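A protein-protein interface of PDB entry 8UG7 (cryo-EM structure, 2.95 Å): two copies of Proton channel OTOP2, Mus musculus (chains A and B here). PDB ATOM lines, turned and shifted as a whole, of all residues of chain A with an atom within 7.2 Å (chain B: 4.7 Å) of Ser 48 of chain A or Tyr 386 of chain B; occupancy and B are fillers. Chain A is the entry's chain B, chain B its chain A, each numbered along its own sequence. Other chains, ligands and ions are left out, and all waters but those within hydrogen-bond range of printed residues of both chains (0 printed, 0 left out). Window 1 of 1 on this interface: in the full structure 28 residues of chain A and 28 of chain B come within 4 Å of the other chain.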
ATOM      1  N   LEU A  41      -1.537  -7.216 -23.448  1.00  0.00           N
ATOM      2  CA  LEU A  41      -1.926  -6.149 -22.532  1.00  0.00           C
ATOM      3  C   LEU A  41      -1.977  -6.649 -21.095  1.00  0.00           C
ATOM      4  O   LEU A  41      -1.555  -5.945 -20.171  1.00  0.00           O
ATOM      5  CB  LEU A  41      -3.276  -5.567 -22.942  1.00  0.00           C
ATOM      6  CG  LEU A  41      -3.832  -4.477 -22.026  1.00  0.00           C
ATOM      7  CD1 LEU A  41      -3.210  -3.128 -22.353  1.00  0.00           C
ATOM      8  CD2 LEU A  41      -5.340  -4.413 -22.125  1.00  0.00           C
ATOM      9  N   LEU A  42      -2.500  -7.859 -20.886  1.00  0.00           N
ATOM     10  CA  LEU A  42      -2.541  -8.420 -19.541  1.00  0.00           C
ATOM     11  C   LEU A  42      -1.140  -8.618 -18.983  1.00  0.00           C
ATOM     12  O   LEU A  42      -0.859  -8.260 -17.834  1.00  0.00           O
ATOM     13  CB  LEU A  42      -3.311  -9.741 -19.555  1.00  0.00           C
ATOM     14  CG  LEU A  42      -3.290 -10.559 -18.266  1.00  0.00           C
ATOM     15  CD1 LEU A  42      -3.809  -9.744 -17.095  1.00  0.00           C
ATOM     16  CD2 LEU A  42      -4.091 -11.836 -18.434  1.00  0.00           C
ATOM     17  N   ALA A  43      -0.239  -9.181 -19.791  1.00  0.00           N
ATOM     18  CA  ALA A  43       1.130  -9.399 -19.332  1.00  0.00           C
ATOM     19  C   ALA A  43       1.849  -8.081 -19.083  1.00  0.00           C
ATOM     20  O   ALA A  43       2.563  -7.937 -18.084  1.00  0.00           O
ATOM     21  CB  ALA A  43       1.894 -10.244 -20.348  1.00  0.00           C
ATOM     22  N   CYS A  44       1.673  -7.107 -19.979  1.00  0.00           N
ATOM     23  CA  CYS A  44       2.385  -5.840 -19.852  1.00  0.00           C
ATOM     24  C   CYS A  44       1.979  -5.095 -18.587  1.00  0.00           C
ATOM     25  O   CYS A  44       2.820  -4.472 -17.931  1.00  0.00           O
ATOM     26  CB  CYS A  44       2.133  -4.976 -21.086  1.00  0.00           C
ATOM     27  SG  CYS A  44       3.010  -5.524 -22.564  1.00  0.00           S
ATOM     28  N   THR A  45       0.693  -5.133 -18.242  1.00  0.00           N
ATOM     29  CA  THR A  45       0.234  -4.478 -17.023  1.00  0.00           C
ATOM     30  C   THR A  45       0.843  -5.123 -15.786  1.00  0.00           C
ATOM     31  O   THR A  45       1.273  -4.425 -14.859  1.00  0.00           O
ATOM     32  CB  THR A  45      -1.293  -4.519 -16.954  1.00  0.00           C
ATOM     33  OG1 THR A  45      -1.841  -3.670 -17.967  1.00  0.00           O
ATOM     34  CG2 THR A  45      -1.774  -4.051 -15.599  1.00  0.00           C
ATOM     35  N   LEU A  46       0.894  -6.456 -15.752  1.00  0.00           N
ATOM     36  CA  LEU A  46       1.497  -7.144 -14.615  1.00  0.00           C
ATOM     37  C   LEU A  46       2.988  -6.850 -14.519  1.00  0.00           C
ATOM     38  O   LEU A  46       3.519  -6.671 -13.418  1.00  0.00           O
ATOM     39  CB  LEU A  46       1.243  -8.646 -14.721  1.00  0.00           C
ATOM     40  CG  LEU A  46      -0.229  -9.062 -14.767  1.00  0.00           C
ATOM     41  CD1 LEU A  46      -0.368 -10.514 -15.172  1.00  0.00           C
ATOM     42  CD2 LEU A  46      -0.888  -8.824 -13.425  1.00  0.00           C
ATOM     43  N   ILE A  47       3.681  -6.806 -15.657  1.00  0.00           N
ATOM     44  CA  ILE A  47       5.106  -6.492 -15.644  1.00  0.00           C
ATOM     45  C   ILE A  47       5.332  -5.053 -15.195  1.00  0.00           C
ATOM     46  O   ILE A  47       6.156  -4.782 -14.313  1.00  0.00           O
ATOM     47  CB  ILE A  47       5.727  -6.749 -17.029  1.00  0.00           C
ATOM     48  CG1 ILE A  47       5.699  -8.240 -17.363  1.00  0.00           C
ATOM     49  CG2 ILE A  47       7.144  -6.221 -17.080  1.00  0.00           C
ATOM     50  CD1 ILE A  47       5.786  -8.524 -18.842  1.00  0.00           C
ATOM     51  N   SER A  48       4.598  -4.110 -15.788  1.00  0.00           N
ATOM     52  CA  SER A  48       4.774  -2.704 -15.437  1.00  0.00           C
ATOM     53  C   SER A  48       4.221  -2.402 -14.052  1.00  0.00           C
ATOM     54  O   SER A  48       4.839  -1.659 -13.279  1.00  0.00           O
ATOM     55  CB  SER A  48       4.111  -1.815 -16.485  1.00  0.00           C
ATOM     56  OG  SER A  48       2.859  -2.347 -16.880  1.00  0.00           O
ATOM     57  N   GLY A  49       3.056  -2.957 -13.721  1.00  0.00           N
ATOM     58  CA  GLY A  49       2.487  -2.719 -12.406  1.00  0.00           C
ATOM     59  C   GLY A  49       3.342  -3.282 -11.288  1.00  0.00           C
ATOM     60  O   GLY A  49       3.514  -2.647 -10.246  1.00  0.00           O
ATOM     61  N   GLY A  50       3.895  -4.478 -11.492  1.00  0.00           N
ATOM     62  CA  GLY A  50       4.704  -5.105 -10.464  1.00  0.00           C
ATOM     63  C   GLY A  50       6.088  -4.509 -10.312  1.00  0.00           C
ATOM     64  O   GLY A  50       6.773  -4.809  -9.330  1.00  0.00           O
ATOM     65  N   ALA A  51       6.508  -3.667 -11.252  1.00  0.00           N
ATOM     66  CA  ALA A  51       7.836  -3.071 -11.219  1.00  0.00           C
ATOM     67  C   ALA A  51       7.840  -1.582 -10.918  1.00  0.00           C
ATOM     68  O   ALA A  51       8.829  -1.080 -10.384  1.00  0.00           O
ATOM     69  CB  ALA A  51       8.555  -3.301 -12.552  1.00  0.00           C
ATOM     70  N   PHE A  52       6.765  -0.866 -11.246  1.00  0.00           N
ATOM     71  CA  PHE A  52       6.718   0.582 -11.096  1.00  0.00           C
ATOM     72  C   PHE A  52       5.804   1.026  -9.962  1.00  0.00           C
ATOM     73  O   PHE A  52       5.456   2.209  -9.879  1.00  0.00           O
ATOM     74  CB  PHE A  52       6.287   1.230 -12.411  1.00  0.00           C
ATOM     75  CG  PHE A  52       7.205   0.927 -13.555  1.00  0.00           C
ATOM     76  CD1 PHE A  52       8.563   1.159 -13.447  1.00  0.00           C
ATOM     77  CD2 PHE A  52       6.714   0.401 -14.734  1.00  0.00           C
ATOM     78  CE1 PHE A  52       9.409   0.882 -14.495  1.00  0.00           C
ATOM     79  CE2 PHE A  52       7.557   0.119 -15.785  1.00  0.00           C
ATOM     80  CZ  PHE A  52       8.906   0.360 -15.667  1.00  0.00           C
ATOM     81  N   ASN A  53       5.407   0.109  -9.087  1.00  0.00           N
ATOM     82  CA  ASN A  53       4.608   0.462  -7.926  1.00  0.00           C
ATOM     83  C   ASN A  53       5.513   0.839  -6.759  1.00  0.00           C
ATOM     84  O   ASN A  53       6.713   0.556  -6.748  1.00  0.00           O
ATOM     85  CB  ASN A  53       3.686  -0.690  -7.537  1.00  0.00           C
ATOM     86  CG  ASN A  53       4.446  -1.912  -7.081  1.00  0.00           C
ATOM     87  OD1 ASN A  53       5.086  -2.591  -7.880  1.00  0.00           O
ATOM     88  ND2 ASN A  53       4.389  -2.196  -5.788  1.00  0.00           N
ATOM     89  N   VAL A  62       6.228 -11.948 -11.616  1.00  0.00           N
ATOM     90  CA  VAL A  62       6.530 -11.691 -13.022  1.00  0.00           C
ATOM     91  C   VAL A  62       7.194 -12.907 -13.656  1.00  0.00           C
ATOM     92  O   VAL A  62       6.859 -13.300 -14.780  1.00  0.00           O
ATOM     93  CB  VAL A  62       7.405 -10.431 -13.154  1.00  0.00           C
ATOM     94  CG1 VAL A  62       7.720 -10.149 -14.616  1.00  0.00           C
ATOM     95  CG2 VAL A  62       6.712  -9.242 -12.515  1.00  0.00           C
ATOM     96  N   MET A 185       9.383  -6.980 -22.941  1.00  0.00           N
ATOM     97  CA  MET A 185       9.090  -5.874 -22.038  1.00  0.00           C
ATOM     98  C   MET A 185       9.662  -6.120 -20.649  1.00  0.00           C
ATOM     99  O   MET A 185      10.174  -5.195 -20.011  1.00  0.00           O
ATOM    100  CB  MET A 185       7.583  -5.635 -21.956  1.00  0.00           C
ATOM    101  CG  MET A 185       7.232  -4.221 -21.536  1.00  0.00           C
ATOM    102  SD  MET A 185       5.613  -4.081 -20.768  1.00  0.00           S
ATOM    103  CE  MET A 185       5.928  -2.803 -19.558  1.00  0.00           C
ATOM    104  N   VAL A 189      12.399  -3.762 -18.783  1.00  0.00           N
ATOM    105  CA  VAL A 189      12.141  -3.219 -17.454  1.00  0.00           C
ATOM    106  C   VAL A 189      13.230  -3.635 -16.474  1.00  0.00           C
ATOM    107  O   VAL A 189      13.601  -2.862 -15.581  1.00  0.00           O
ATOM    108  CB  VAL A 189      10.742  -3.651 -16.977  1.00  0.00           C
ATOM    109  CG1 VAL A 189      10.579  -3.419 -15.490  1.00  0.00           C
ATOM    110  CG2 VAL A 189       9.672  -2.907 -17.757  1.00  0.00           C
ATOM    111  N   ALA B 382      -6.993  -2.416 -19.264  1.00  0.00           N
ATOM    112  CA  ALA B 382      -5.766  -1.998 -18.595  1.00  0.00           C
ATOM    113  C   ALA B 382      -6.063  -1.316 -17.267  1.00  0.00           C
ATOM    114  O   ALA B 382      -5.358  -1.541 -16.278  1.00  0.00           O
ATOM    115  CB  ALA B 382      -4.960  -1.077 -19.506  1.00  0.00           C
ATOM    116  N   ILE B 383      -7.101  -0.477 -17.224  1.00  0.00           N
ATOM    117  CA  ILE B 383      -7.487   0.164 -15.969  1.00  0.00           C
ATOM    118  C   ILE B 383      -7.872  -0.890 -14.941  1.00  0.00           C
ATOM    119  O   ILE B 383      -7.478  -0.820 -13.771  1.00  0.00           O
ATOM    120  CB  ILE B 383      -8.632   1.164 -16.203  1.00  0.00           C
ATOM    121  CG1 ILE B 383      -8.163   2.337 -17.063  1.00  0.00           C
ATOM    122  CG2 ILE B 383      -9.175   1.674 -14.878  1.00  0.00           C
ATOM    123  CD1 ILE B 383      -7.394   3.382 -16.302  1.00  0.00           C
ATOM    124  N   SER B 384      -8.651  -1.886 -15.367  1.00  0.00           N
ATOM    125  CA  SER B 384      -9.061  -2.952 -14.460  1.00  0.00           C
ATOM    126  C   SER B 384      -7.876  -3.802 -14.024  1.00  0.00           C
ATOM    127  O   SER B 384      -7.749  -4.134 -12.842  1.00  0.00           O
ATOM    128  CB  SER B 384     -10.122  -3.819 -15.128  1.00  0.00           C
ATOM    129  OG  SER B 384     -11.355  -3.130 -15.220  1.00  0.00           O
ATOM    130  N   TYR B 385      -6.998  -4.166 -14.962  1.00  0.00           N
ATOM    131  CA  TYR B 385      -5.835  -4.977 -14.614  1.00  0.00           C
ATOM    132  C   TYR B 385      -4.943  -4.250 -13.618  1.00  0.00           C
ATOM    133  O   TYR B 385      -4.477  -4.837 -12.638  1.00  0.00           O
ATOM    134  CB  TYR B 385      -5.039  -5.337 -15.868  1.00  0.00           C
ATOM    135  CG  TYR B 385      -5.743  -6.254 -16.834  1.00  0.00           C
ATOM    136  CD1 TYR B 385      -6.713  -7.144 -16.404  1.00  0.00           C
ATOM    137  CD2 TYR B 385      -5.426  -6.232 -18.184  1.00  0.00           C
ATOM    138  CE1 TYR B 385      -7.353  -7.982 -17.292  1.00  0.00           C
ATOM    139  CE2 TYR B 385      -6.059  -7.065 -19.078  1.00  0.00           C
ATOM    140  CZ  TYR B 385      -7.021  -7.937 -18.628  1.00  0.00           C
ATOM    141  OH  TYR B 385      -7.651  -8.766 -19.522  1.00  0.00           O
ATOM    142  N   TYR B 386      -4.695  -2.962 -13.855  1.00  0.00           N
ATOM    143  CA  TYR B 386      -3.898  -2.179 -12.921  1.00  0.00           C
ATOM    144  C   TYR B 386      -4.599  -2.056 -11.575  1.00  0.00           C
ATOM    145  O   TYR B 386      -3.950  -2.067 -10.523  1.00  0.00           O
ATOM    146  CB  TYR B 386      -3.617  -0.795 -13.502  1.00  0.00           C
ATOM    147  CG  TYR B 386      -2.393  -0.737 -14.382  1.00  0.00           C
ATOM    148  CD1 TYR B 386      -1.131  -0.980 -13.864  1.00  0.00           C
ATOM    149  CD2 TYR B 386      -2.500  -0.432 -15.730  1.00  0.00           C
ATOM    150  CE1 TYR B 386      -0.013  -0.926 -14.664  1.00  0.00           C
ATOM    151  CE2 TYR B 386      -1.388  -0.376 -16.539  1.00  0.00           C
ATOM    152  CZ  TYR B 386      -0.147  -0.624 -16.000  1.00  0.00           C
ATOM    153  OH  TYR B 386       0.968  -0.569 -16.802  1.00  0.00           O
ATOM    154  N   SER B 387      -5.926  -1.925 -11.591  1.00  0.00           N
ATOM    155  CA  SER B 387      -6.684  -1.820 -10.351  1.00  0.00           C
ATOM    156  C   SER B 387      -6.603  -3.104  -9.536  1.00  0.00           C
ATOM    157  O   SER B 387      -6.466  -3.058  -8.308  1.00  0.00           O
ATOM    158  CB  SER B 387      -8.138  -1.481 -10.660  1.00  0.00           C
ATOM    159  OG  SER B 387      -8.282  -0.112 -10.987  1.00  0.00           O
ATOM    160  N   ILE B 388      -6.687  -4.257 -10.200  1.00  0.00           N
ATOM    161  CA  ILE B 388      -6.757  -5.531  -9.486  1.00  0.00           C
ATOM    162  C   ILE B 388      -5.482  -5.771  -8.688  1.00  0.00           C
ATOM    163  O   ILE B 388      -5.529  -6.116  -7.502  1.00  0.00           O
ATOM    164  CB  ILE B 388      -7.031  -6.682 -10.469  1.00  0.00           C
ATOM    165  CG1 ILE B 388      -8.475  -6.625 -10.964  1.00  0.00           C
ATOM    166  CG2 ILE B 388      -6.748  -8.019  -9.813  1.00  0.00           C
ATOM    167  CD1 ILE B 388      -8.723  -7.454 -12.193  1.00  0.00           C
ATOM    168  N   VAL B 389      -4.348  -5.545  -9.325  1.00  0.00           N
ATOM    169  CA  VAL B 389      -3.041  -5.784  -8.663  1.00  0.00           C
ATOM    170  C   VAL B 389      -2.925  -4.801  -7.516  1.00  0.00           C
ATOM    171  O   VAL B 389      -2.416  -5.190  -6.459  1.00  0.00           O
ATOM    172  CB  VAL B 389      -1.840  -5.750  -9.637  1.00  0.00           C
ATOM    173  CG1 VAL B 389      -2.091  -6.469 -10.943  1.00  0.00           C
ATOM    174  CG2 VAL B 389      -1.212  -4.385  -9.839  1.00  0.00           C
ATOM    175  N   ALA B 390      -3.424  -3.602  -7.707  1.00  0.00           N
ATOM    176  CA  ALA B 390      -3.306  -2.579  -6.677  1.00  0.00           C
ATOM    177  C   ALA B 390      -4.155  -2.912  -5.461  1.00  0.00           C
ATOM    178  O   ALA B 390      -3.947  -2.342  -4.385  1.00  0.00           O
ATOM    179  CB  ALA B 390      -3.698  -1.213  -7.240  1.00  0.00           C
ATOM    180  N   TYR B 529       0.578   3.183  -7.106  1.00  0.00           N
ATOM    181  CA  TYR B 529       1.415   3.557  -8.236  1.00  0.00           C
ATOM    182  C   TYR B 529       2.001   4.956  -8.123  1.00  0.00           C
ATOM    183  O   TYR B 529       2.916   5.289  -8.883  1.00  0.00           O
ATOM    184  CB  TYR B 529       0.622   3.470  -9.543  1.00  0.00           C
ATOM    185  CG  TYR B 529       0.019   2.119  -9.828  1.00  0.00           C
ATOM    186  CD1 TYR B 529       0.807   1.064 -10.259  1.00  0.00           C
ATOM    187  CD2 TYR B 529      -1.340   1.903  -9.680  1.00  0.00           C
ATOM    188  CE1 TYR B 529       0.257  -0.171 -10.526  1.00  0.00           C
ATOM    189  CE2 TYR B 529      -1.898   0.676  -9.943  1.00  0.00           C
ATOM    190  CZ  TYR B 529      -1.097  -0.357 -10.364  1.00  0.00           C
ATOM    191  OH  TYR B 529      -1.655  -1.583 -10.629  1.00  0.00           O
ATOM    192  N   TRP B 534      -0.298   6.881 -12.009  1.00  0.00           N
ATOM    193  CA  TRP B 534      -1.712   6.565 -12.180  1.00  0.00           C
ATOM    194  C   TRP B 534      -2.405   7.588 -13.067  1.00  0.00           C
ATOM    195  O   TRP B 534      -3.261   7.228 -13.882  1.00  0.00           O
ATOM    196  CB  TRP B 534      -2.407   6.477 -10.822  1.00  0.00           C
ATOM    197  CG  TRP B 534      -3.826   6.029 -10.939  1.00  0.00           C
ATOM    198  CD1 TRP B 534      -4.940   6.739 -10.608  1.00  0.00           C
ATOM    199  CD2 TRP B 534      -4.288   4.768 -11.438  1.00  0.00           C
ATOM    200  NE1 TRP B 534      -6.067   6.000 -10.866  1.00  0.00           N
ATOM    201  CE2 TRP B 534      -5.694   4.785 -11.375  1.00  0.00           C
ATOM    202  CE3 TRP B 534      -3.649   3.627 -11.927  1.00  0.00           C
ATOM    203  CZ2 TRP B 534      -6.469   3.707 -11.783  1.00  0.00           C
ATOM    204  CZ3 TRP B 534      -4.420   2.559 -12.331  1.00  0.00           C
ATOM    205  CH2 TRP B 534      -5.815   2.604 -12.256  1.00  0.00           C
ATOM    206  N   ILE B 537      -1.753   6.648 -16.486  1.00  0.00           N
ATOM    207  CA  ILE B 537      -2.489   5.456 -16.901  1.00  0.00           C
ATOM    208  C   ILE B 537      -3.918   5.819 -17.284  1.00  0.00           C
ATOM    209  O   ILE B 537      -4.417   5.414 -18.340  1.00  0.00           O
ATOM    210  CB  ILE B 537      -2.456   4.392 -15.789  1.00  0.00           C
ATOM    211  CG1 ILE B 537      -1.061   3.781 -15.675  1.00  0.00           C
ATOM    212  CG2 ILE B 537      -3.489   3.312 -16.051  1.00  0.00           C
ATOM    213  CD1 ILE B 537      -0.874   2.925 -14.445  1.00  0.00           C
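OG of Ser 48 of chain A lies within hydrogen-bond range of OH of Tyr 386 of chain B, at 2.6 Å.
The side-chain hydroxyl of Ser 48 of chain A is in hydrogen-bond range of the backbone carbonyl oxygen of Thr 45 of chain A (3.3 Å).
The backbone carbonyl oxygen (O) of Leu 41 of chain A lies within hydrogen-bond range of the side-chain hydroxyl (OG1) of Thr 45 of chain A, 3.2 Å away.
The side-chain amide oxygen (OD1) of Asn 53 of chain A sits close to the backbone carbonyl oxygen (O) of Gly 49 of chain A (2.8 Å).
Among the printed residues, merely in contact across the chains: Thr 45 of chain A with Tyr 385 of chain B, Thr 45 of chain A with Tyr 386 of chain B, Leu 46 of chain A with Val 389 of chain B, Leu 42 of chain A with Tyr 385 of chain B, Gly 49 of chain A with Tyr 386 of chain B, Leu 41 of chain A with Ala 382 of chain B and Gly 49 of chain A with Tyr 529 of chain B.
Printed residues of chain B within 4 Å of Thr 45 of chain A: Tyr 385 and Tyr 386.
Of the printed residues of chain B, Leu 46 of chain A touches Val 389 (3.6 Å).
Ser 48 of chain A touches one residue of chain B.
Asn 53 of chain A touches none of the printed residues of chain B.
Val 189 of chain A touches none of the printed residues of chain B.
Printed residues of chain A within 4 Å of Ala 382 of chain B: Leu 41.
Tyr 386 of chain B touches just these residues of chain A: Thr 45 (3.6 Å), Ser 48 (2.6 Å) and Gly 49 (3.8 Å).
Hydrophobic or aromatic side chains of chain B within 4 Å of the printed part of chain A: Ala 382, Tyr 385, Tyr 386, Val 389 and Tyr 529.
Along chain A the printed residues that touch a printed residue of chain B span positions 41 to 49.
Among the printed residues, 8 pairs touch across the chains.
No position is printed for both chains.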
